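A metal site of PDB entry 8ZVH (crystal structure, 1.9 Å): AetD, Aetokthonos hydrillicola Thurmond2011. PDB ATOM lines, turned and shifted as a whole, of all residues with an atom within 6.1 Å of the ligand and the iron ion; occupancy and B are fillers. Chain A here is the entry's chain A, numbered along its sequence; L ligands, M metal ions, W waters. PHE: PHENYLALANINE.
Within 4 Å of the iron ion: His 90, His 183 and Glu 187.
The side-chain carboxylate (OE2) of Glu 151 lies close to the side-chain carboxylate (OE2) of Glu 187, at 2.5 Å. ND1 of His 183 lies within hydrogen-bond range of O of Tyr 178 (2.8 Å).
The side-chain hydroxyl (OH) of Tyr 178 lies within hydrogen-bond range of an oxygen (O) of the ligand (2.6 Å).
Residues that only touch the ligand: Phe 55 (3.2 Å), Phe 59 (3.4 Å), Met 150 (3.2 Å), Gly 154 (3.2 Å), Ile 157 (3.999 Å) and Phe 158 (3.6 Å). Hydrophobic or aromatic side chains within 4 Å of the ligand: Phe 55, Phe 59, His 90, Met 150, Ile 157, Phe 158, Tyr 178 and His 183. Along chain A the residues within 4 Å of the ligand span positions 55 to 187. The nearest printed residue that does not touch the ligand is Glu 151 (4.2 Å).
Water W1 lies within hydrogen-bond range of the side-chain carboxylate (OE2) of Glu 187 (2.5 Å) and the backbone carbonyl oxygen (O) of Asp 87 (3.3 Å). Water W2 lies within hydrogen-bond range of O of the ligand (2.6 Å), O of Ala 56 (2.9 Å) and N of Trp 91 (3.5 Å).
The iron ion is bound by water W1, N of the ligand, OE1 of Glu 187, NE2 of His 183, OXT of the ligand and ND1 of His 90. The iron ion has six donor atoms within binding distance.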
ATOM      1  N   ILE A  52       3.031 -20.329  -4.663  1.00  0.00           N
ATOM      2  CA  ILE A  52       4.046 -20.702  -5.703  1.00  0.00           C
ATOM      3  C   ILE A  52       3.351 -20.727  -7.085  1.00  0.00           C
ATOM      4  O   ILE A  52       4.069 -20.574  -8.105  1.00  0.00           O
ATOM      5  CB  ILE A  52       4.758 -22.020  -5.345  1.00  0.00           C
ATOM      6  CG1 ILE A  52       5.496 -21.930  -4.008  1.00  0.00           C
ATOM      7  CG2 ILE A  52       5.712 -22.423  -6.446  1.00  0.00           C
ATOM      8  CD1 ILE A  52       5.820 -23.292  -3.429  1.00  0.00           C
ATOM      9  N   PHE A  55       4.187 -18.326  -9.697  1.00  0.00           N
ATOM     10  CA  PHE A  55       5.644 -18.423 -10.052  1.00  0.00           C
ATOM     11  C   PHE A  55       5.926 -19.692 -10.872  1.00  0.00           C
ATOM     12  O   PHE A  55       6.670 -19.611 -11.865  1.00  0.00           O
ATOM     13  CB  PHE A  55       6.567 -18.411  -8.825  1.00  0.00           C
ATOM     14  CG  PHE A  55       7.964 -18.831  -9.175  1.00  0.00           C
ATOM     15  CD1 PHE A  55       8.847 -17.925  -9.740  1.00  0.00           C
ATOM     16  CD2 PHE A  55       8.358 -20.153  -9.069  1.00  0.00           C
ATOM     17  CE1 PHE A  55      10.106 -18.315 -10.169  1.00  0.00           C
ATOM     18  CE2 PHE A  55       9.607 -20.553  -9.522  1.00  0.00           C
ATOM     19  CZ  PHE A  55      10.468 -19.643 -10.079  1.00  0.00           C
ATOM     20  N   ALA A  56       5.438 -20.836 -10.422  1.00  0.00           N
ATOM     21  CA  ALA A  56       5.787 -22.163 -10.992  1.00  0.00           C
ATOM     22  C   ALA A  56       5.491 -22.202 -12.494  1.00  0.00           C
ATOM     23  O   ALA A  56       6.340 -22.639 -13.258  1.00  0.00           O
ATOM     24  CB  ALA A  56       5.019 -23.242 -10.288  1.00  0.00           C
ATOM     25  N   PHE A  59       7.571 -19.831 -14.521  1.00  0.00           N
ATOM     26  CA  PHE A  59       8.933 -20.373 -14.651  1.00  0.00           C
ATOM     27  C   PHE A  59       9.018 -21.330 -15.863  1.00  0.00           C
ATOM     28  O   PHE A  59      10.056 -21.347 -16.593  1.00  0.00           O
ATOM     29  CB  PHE A  59       9.362 -21.074 -13.373  1.00  0.00           C
ATOM     30  CG  PHE A  59      10.793 -21.509 -13.452  1.00  0.00           C
ATOM     31  CD1 PHE A  59      11.813 -20.585 -13.326  1.00  0.00           C
ATOM     32  CD2 PHE A  59      11.120 -22.845 -13.672  1.00  0.00           C
ATOM     33  CE1 PHE A  59      13.142 -20.979 -13.438  1.00  0.00           C
ATOM     34  CE2 PHE A  59      12.448 -23.230 -13.779  1.00  0.00           C
ATOM     35  CZ  PHE A  59      13.451 -22.304 -13.680  1.00  0.00           C
ATOM     36  N   ASP A  87      13.954 -28.621 -16.932  1.00  0.00           N
ATOM     37  CA  ASP A  87      13.549 -27.701 -15.817  1.00  0.00           C
ATOM     38  C   ASP A  87      12.134 -27.156 -16.060  1.00  0.00           C
ATOM     39  O   ASP A  87      11.449 -26.774 -15.072  1.00  0.00           O
ATOM     40  CB  ASP A  87      14.519 -26.537 -15.713  1.00  0.00           C
ATOM     41  CG  ASP A  87      15.948 -26.929 -15.350  1.00  0.00           C
ATOM     42  OD1 ASP A  87      16.122 -27.971 -14.709  1.00  0.00           O
ATOM     43  OD2 ASP A  87      16.877 -26.142 -15.704  1.00  0.00           O
ATOM     44  N   HIS A  90       8.730 -29.243 -14.329  1.00  0.00           N
ATOM     45  CA  HIS A  90       8.499 -29.361 -12.879  1.00  0.00           C
ATOM     46  C   HIS A  90       7.122 -28.798 -12.489  1.00  0.00           C
ATOM     47  O   HIS A  90       6.645 -29.080 -11.401  1.00  0.00           O
ATOM     48  CB  HIS A  90       9.637 -28.700 -12.102  1.00  0.00           C
ATOM     49  CG  HIS A  90      10.970 -29.313 -12.395  1.00  0.00           C
ATOM     50  ND1 HIS A  90      12.133 -28.768 -11.893  1.00  0.00           N
ATOM     51  CD2 HIS A  90      11.340 -30.373 -13.159  1.00  0.00           C
ATOM     52  CE1 HIS A  90      13.165 -29.469 -12.311  1.00  0.00           C
ATOM     53  NE2 HIS A  90      12.721 -30.457 -13.093  1.00  0.00           N
ATOM     54  N   TRP A  91       6.483 -28.025 -13.374  1.00  0.00           N
ATOM     55  CA  TRP A  91       5.191 -27.396 -13.022  1.00  0.00           C
ATOM     56  C   TRP A  91       4.125 -28.462 -12.774  1.00  0.00           C
ATOM     57  O   TRP A  91       3.260 -28.244 -11.938  1.00  0.00           O
ATOM     58  CB  TRP A  91       4.802 -26.405 -14.094  1.00  0.00           C
ATOM     59  CG  TRP A  91       4.578 -27.079 -15.410  1.00  0.00           C
ATOM     60  CD1 TRP A  91       5.521 -27.446 -16.316  1.00  0.00           C
ATOM     61  CD2 TRP A  91       3.309 -27.392 -15.990  1.00  0.00           C
ATOM     62  NE1 TRP A  91       4.929 -27.997 -17.415  1.00  0.00           N
ATOM     63  CE2 TRP A  91       3.567 -27.992 -17.243  1.00  0.00           C
ATOM     64  CE3 TRP A  91       1.990 -27.261 -15.568  1.00  0.00           C
ATOM     65  CZ2 TRP A  91       2.552 -28.437 -18.087  1.00  0.00           C
ATOM     66  CZ3 TRP A  91       0.980 -27.725 -16.398  1.00  0.00           C
ATOM     67  CH2 TRP A  91       1.271 -28.319 -17.634  1.00  0.00           C
ATOM     68  N   TRP A  93       4.767 -31.252 -11.306  1.00  0.00           N
ATOM     69  CA  TRP A  93       5.082 -31.687  -9.927  1.00  0.00           C
ATOM     70  C   TRP A  93       4.394 -30.693  -8.970  1.00  0.00           C
ATOM     71  O   TRP A  93       3.777 -31.146  -8.015  1.00  0.00           O
ATOM     72  CB  TRP A  93       6.578 -31.790  -9.688  1.00  0.00           C
ATOM     73  CG  TRP A  93       7.307 -32.726 -10.595  1.00  0.00           C
ATOM     74  CD1 TRP A  93       6.790 -33.697 -11.420  1.00  0.00           C
ATOM     75  CD2 TRP A  93       8.733 -32.775 -10.759  1.00  0.00           C
ATOM     76  NE1 TRP A  93       7.803 -34.343 -12.075  1.00  0.00           N
ATOM     77  CE2 TRP A  93       9.007 -33.811 -11.682  1.00  0.00           C
ATOM     78  CE3 TRP A  93       9.803 -32.089 -10.178  1.00  0.00           C
ATOM     79  CZ2 TRP A  93      10.309 -34.112 -12.075  1.00  0.00           C
ATOM     80  CZ3 TRP A  93      11.086 -32.421 -10.543  1.00  0.00           C
ATOM     81  CH2 TRP A  93      11.331 -33.399 -11.510  1.00  0.00           C
ATOM     82  N   PHE A  94       4.467 -29.389  -9.256  1.00  0.00           N
ATOM     83  CA  PHE A  94       3.789 -28.351  -8.453  1.00  0.00           C
ATOM     84  C   PHE A  94       2.299 -28.712  -8.297  1.00  0.00           C
ATOM     85  O   PHE A  94       1.723 -28.670  -7.204  1.00  0.00           O
ATOM     86  CB  PHE A  94       3.989 -26.960  -9.042  1.00  0.00           C
ATOM     87  CG  PHE A  94       3.050 -25.966  -8.432  1.00  0.00           C
ATOM     88  CD1 PHE A  94       3.261 -25.486  -7.144  1.00  0.00           C
ATOM     89  CD2 PHE A  94       1.885 -25.581  -9.091  1.00  0.00           C
ATOM     90  CE1 PHE A  94       2.343 -24.650  -6.517  1.00  0.00           C
ATOM     91  CE2 PHE A  94       0.982 -24.729  -8.470  1.00  0.00           C
ATOM     92  CZ  PHE A  94       1.204 -24.271  -7.201  1.00  0.00           C
ATOM     93  N   LEU A 127       8.625 -12.198 -10.997  1.00  0.00           N
ATOM     94  CA  LEU A 127      10.048 -12.655 -10.983  1.00  0.00           C
ATOM     95  C   LEU A 127      10.494 -13.123 -12.386  1.00  0.00           C
ATOM     96  O   LEU A 127      11.501 -12.580 -12.925  1.00  0.00           O
ATOM     97  CB  LEU A 127      10.252 -13.745  -9.916  1.00  0.00           C
ATOM     98  CG  LEU A 127      11.668 -14.335  -9.933  1.00  0.00           C
ATOM     99  CD1 LEU A 127      12.730 -13.282  -9.682  1.00  0.00           C
ATOM    100  CD2 LEU A 127      11.793 -15.436  -8.903  1.00  0.00           C
ATOM    101  N   MET A 150      19.938 -17.733 -10.640  1.00  0.00           N
ATOM    102  CA  MET A 150      18.512 -18.058 -10.394  1.00  0.00           C
ATOM    103  C   MET A 150      18.451 -19.439  -9.736  1.00  0.00           C
ATOM    104  O   MET A 150      17.719 -19.600  -8.723  1.00  0.00           O
ATOM    105  CB  MET A 150      17.752 -18.128 -11.730  1.00  0.00           C
ATOM    106  CG  MET A 150      16.851 -16.981 -11.971  1.00  0.00           C
ATOM    107  SD  MET A 150      15.487 -17.046 -10.825  1.00  0.00           S
ATOM    108  CE  MET A 150      14.288 -17.921 -11.824  1.00  0.00           C
ATOM    109  N   GLU A 151      19.157 -20.399 -10.329  1.00  0.00           N
ATOM    110  CA  GLU A 151      19.137 -21.809  -9.873  1.00  0.00           C
ATOM    111  C   GLU A 151      19.754 -21.902  -8.483  1.00  0.00           C
ATOM    112  O   GLU A 151      19.270 -22.745  -7.651  1.00  0.00           O
ATOM    113  CB  GLU A 151      19.829 -22.698 -10.908  1.00  0.00           C
ATOM    114  CG  GLU A 151      18.906 -23.069 -12.060  1.00  0.00           C
ATOM    115  CD  GLU A 151      17.802 -24.034 -11.632  1.00  0.00           C
ATOM    116  OE1 GLU A 151      17.740 -24.423 -10.443  1.00  0.00           O
ATOM    117  OE2 GLU A 151      17.043 -24.421 -12.467  1.00  0.00           O
ATOM    118  N   THR A 152      20.740 -21.059  -8.187  1.00  0.00           N
ATOM    119  CA  THR A 152      21.385 -21.013  -6.850  1.00  0.00           C
ATOM    120  C   THR A 152      20.307 -20.677  -5.817  1.00  0.00           C
ATOM    121  O   THR A 152      20.213 -21.410  -4.841  1.00  0.00           O
ATOM    122  CB  THR A 152      22.583 -20.059  -6.803  1.00  0.00           C
ATOM    123  OG1 THR A 152      23.567 -20.513  -7.730  1.00  0.00           O
ATOM    124  CG2 THR A 152      23.185 -19.948  -5.426  1.00  0.00           C
ATOM    125  N   ALA A 153      19.482 -19.654  -6.071  1.00  0.00           N
ATOM    126  CA  ALA A 153      18.328 -19.281  -5.236  1.00  0.00           C
ATOM    127  C   ALA A 153      17.297 -20.412  -5.189  1.00  0.00           C
ATOM    128  O   ALA A 153      16.781 -20.697  -4.084  1.00  0.00           O
ATOM    129  CB  ALA A 153      17.733 -17.985  -5.732  1.00  0.00           C
ATOM    130  N   GLY A 154      16.920 -20.995  -6.332  1.00  0.00           N
ATOM    131  CA  GLY A 154      15.968 -22.121  -6.377  1.00  0.00           C
ATOM    132  C   GLY A 154      16.397 -23.255  -5.452  1.00  0.00           C
ATOM    133  O   GLY A 154      15.537 -23.843  -4.709  1.00  0.00           O
ATOM    134  N   LEU A 155      17.672 -23.619  -5.505  1.00  0.00           N
ATOM    135  CA  LEU A 155      18.185 -24.782  -4.734  1.00  0.00           C
ATOM    136  C   LEU A 155      18.061 -24.449  -3.237  1.00  0.00           C
ATOM    137  O   LEU A 155      17.680 -25.342  -2.460  1.00  0.00           O
ATOM    138  CB  LEU A 155      19.624 -25.112  -5.131  1.00  0.00           C
ATOM    139  CG  LEU A 155      19.816 -25.631  -6.555  1.00  0.00           C
ATOM    140  CD1 LEU A 155      21.229 -26.152  -6.730  1.00  0.00           C
ATOM    141  CD2 LEU A 155      18.785 -26.716  -6.904  1.00  0.00           C
ATOM    142  N   ILE A 157      15.670 -22.455  -1.944  1.00  0.00           N
ATOM    143  CA  ILE A 157      14.203 -22.457  -1.701  1.00  0.00           C
ATOM    144  C   ILE A 157      13.739 -23.904  -1.504  1.00  0.00           C
ATOM    145  O   ILE A 157      12.998 -24.181  -0.555  1.00  0.00           O
ATOM    146  CB  ILE A 157      13.440 -21.780  -2.862  1.00  0.00           C
ATOM    147  CG1 ILE A 157      13.648 -20.256  -2.902  1.00  0.00           C
ATOM    148  CG2 ILE A 157      11.984 -22.152  -2.740  1.00  0.00           C
ATOM    149  CD1 ILE A 157      13.206 -19.621  -4.230  1.00  0.00           C
ATOM    150  N   PHE A 158      14.066 -24.766  -2.455  1.00  0.00           N
ATOM    151  CA  PHE A 158      13.544 -26.135  -2.521  1.00  0.00           C
ATOM    152  C   PHE A 158      14.233 -27.028  -1.502  1.00  0.00           C
ATOM    153  O   PHE A 158      13.585 -27.920  -0.975  1.00  0.00           O
ATOM    154  CB  PHE A 158      13.568 -26.624  -3.970  1.00  0.00           C
ATOM    155  CG  PHE A 158      12.420 -26.003  -4.709  1.00  0.00           C
ATOM    156  CD1 PHE A 158      11.129 -26.470  -4.493  1.00  0.00           C
ATOM    157  CD2 PHE A 158      12.596 -24.849  -5.435  1.00  0.00           C
ATOM    158  CE1 PHE A 158      10.043 -25.838  -5.083  1.00  0.00           C
ATOM    159  CE2 PHE A 158      11.501 -24.221  -6.020  1.00  0.00           C
ATOM    160  CZ  PHE A 158      10.234 -24.724  -5.856  1.00  0.00           C
ATOM    161  N   TYR A 178       7.390 -32.102  -5.858  1.00  0.00           N
ATOM    162  CA  TYR A 178       7.799 -30.682  -5.980  1.00  0.00           C
ATOM    163  C   TYR A 178       8.517 -30.197  -4.725  1.00  0.00           C
ATOM    164  O   TYR A 178       9.641 -29.686  -4.849  1.00  0.00           O
ATOM    165  CB  TYR A 178       6.579 -29.823  -6.345  1.00  0.00           C
ATOM    166  CG  TYR A 178       6.896 -28.428  -6.821  1.00  0.00           C
ATOM    167  CD1 TYR A 178       7.463 -28.202  -8.054  1.00  0.00           C
ATOM    168  CD2 TYR A 178       6.619 -27.323  -6.015  1.00  0.00           C
ATOM    169  CE1 TYR A 178       7.769 -26.931  -8.497  1.00  0.00           C
ATOM    170  CE2 TYR A 178       6.882 -26.035  -6.456  1.00  0.00           C
ATOM    171  CZ  TYR A 178       7.485 -25.839  -7.692  1.00  0.00           C
ATOM    172  OH  TYR A 178       7.780 -24.585  -8.148  1.00  0.00           O
ATOM    173  N   HIS A 183      13.286 -33.377  -6.384  1.00  0.00           N
ATOM    174  CA  HIS A 183      13.271 -32.122  -7.179  1.00  0.00           C
ATOM    175  C   HIS A 183      14.628 -31.438  -7.078  1.00  0.00           C
ATOM    176  O   HIS A 183      15.192 -31.083  -8.134  1.00  0.00           O
ATOM    177  CB  HIS A 183      12.107 -31.242  -6.715  1.00  0.00           C
ATOM    178  CG  HIS A 183      11.938 -30.005  -7.529  1.00  0.00           C
ATOM    179  ND1 HIS A 183      11.061 -29.026  -7.160  1.00  0.00           N
ATOM    180  CD2 HIS A 183      12.546 -29.553  -8.644  1.00  0.00           C
ATOM    181  CE1 HIS A 183      11.098 -28.035  -8.031  1.00  0.00           C
ATOM    182  NE2 HIS A 183      11.984 -28.320  -8.947  1.00  0.00           N
ATOM    183  N   GLU A 187      17.245 -31.190 -10.309  1.00  0.00           N
ATOM    184  CA  GLU A 187      17.494 -29.750 -10.635  1.00  0.00           C
ATOM    185  C   GLU A 187      19.001 -29.426 -10.586  1.00  0.00           C
ATOM    186  O   GLU A 187      19.478 -28.772 -11.533  1.00  0.00           O
ATOM    187  CB  GLU A 187      16.726 -28.842  -9.666  1.00  0.00           C
ATOM    188  CG  GLU A 187      16.662 -27.377 -10.093  1.00  0.00           C
ATOM    189  CD  GLU A 187      15.343 -26.962 -10.733  1.00  0.00           C
ATOM    190  OE1 GLU A 187      14.324 -27.577 -10.373  1.00  0.00           O
ATOM    191  OE2 GLU A 187      15.345 -26.032 -11.606  1.00  0.00           O
ATOM    192  N   SER A 225      14.468 -12.426  -6.044  1.00  0.00           N
ATOM    193  CA  SER A 225      14.236 -13.671  -5.273  1.00  0.00           C
ATOM    194  C   SER A 225      13.872 -13.331  -3.834  1.00  0.00           C
ATOM    195  O   SER A 225      12.882 -13.874  -3.351  1.00  0.00           O
ATOM    196  CB  SER A 225      15.413 -14.596  -5.379  1.00  0.00           C
ATOM    197  OG  SER A 225      15.637 -14.971  -6.744  1.00  0.00           O
HETATM  198  N   PHE L   1      12.656 -25.387  -9.398  1.00  0.00           N
HETATM  199  CA  PHE L   1      11.532 -24.422  -9.568  1.00  0.00           C
HETATM  200  C   PHE L   1      10.344 -25.154 -10.213  1.00  0.00           C
HETATM  201  O   PHE L   1       9.265 -24.541 -10.329  1.00  0.00           O
HETATM  202  CB  PHE L   1      11.968 -23.234 -10.442  1.00  0.00           C
HETATM  203  CG  PHE L   1      12.896 -22.233  -9.809  1.00  0.00           C
HETATM  204  CD1 PHE L   1      12.553 -21.560  -8.658  1.00  0.00           C
HETATM  205  CD2 PHE L   1      14.140 -21.987 -10.373  1.00  0.00           C
HETATM  206  CE1 PHE L   1      13.394 -20.606  -8.101  1.00  0.00           C
HETATM  207  CE2 PHE L   1      14.988 -21.045  -9.814  1.00  0.00           C
HETATM  208  CZ  PHE L   1      14.613 -20.361  -8.687  1.00  0.00           C
HETATM  209  OXT PHE L   1      10.379 -26.362 -10.627  1.00  0.00           O
HETATM  210 FE    FE M   1      12.344 -27.038 -10.534  1.00  0.00          FE
HETATM  211  O   HOH W   1      12.889 -26.071 -12.223  1.00  0.00           O
HETATM  212  O   HOH W   2       7.859 -24.941 -12.457  1.00  0.00           O
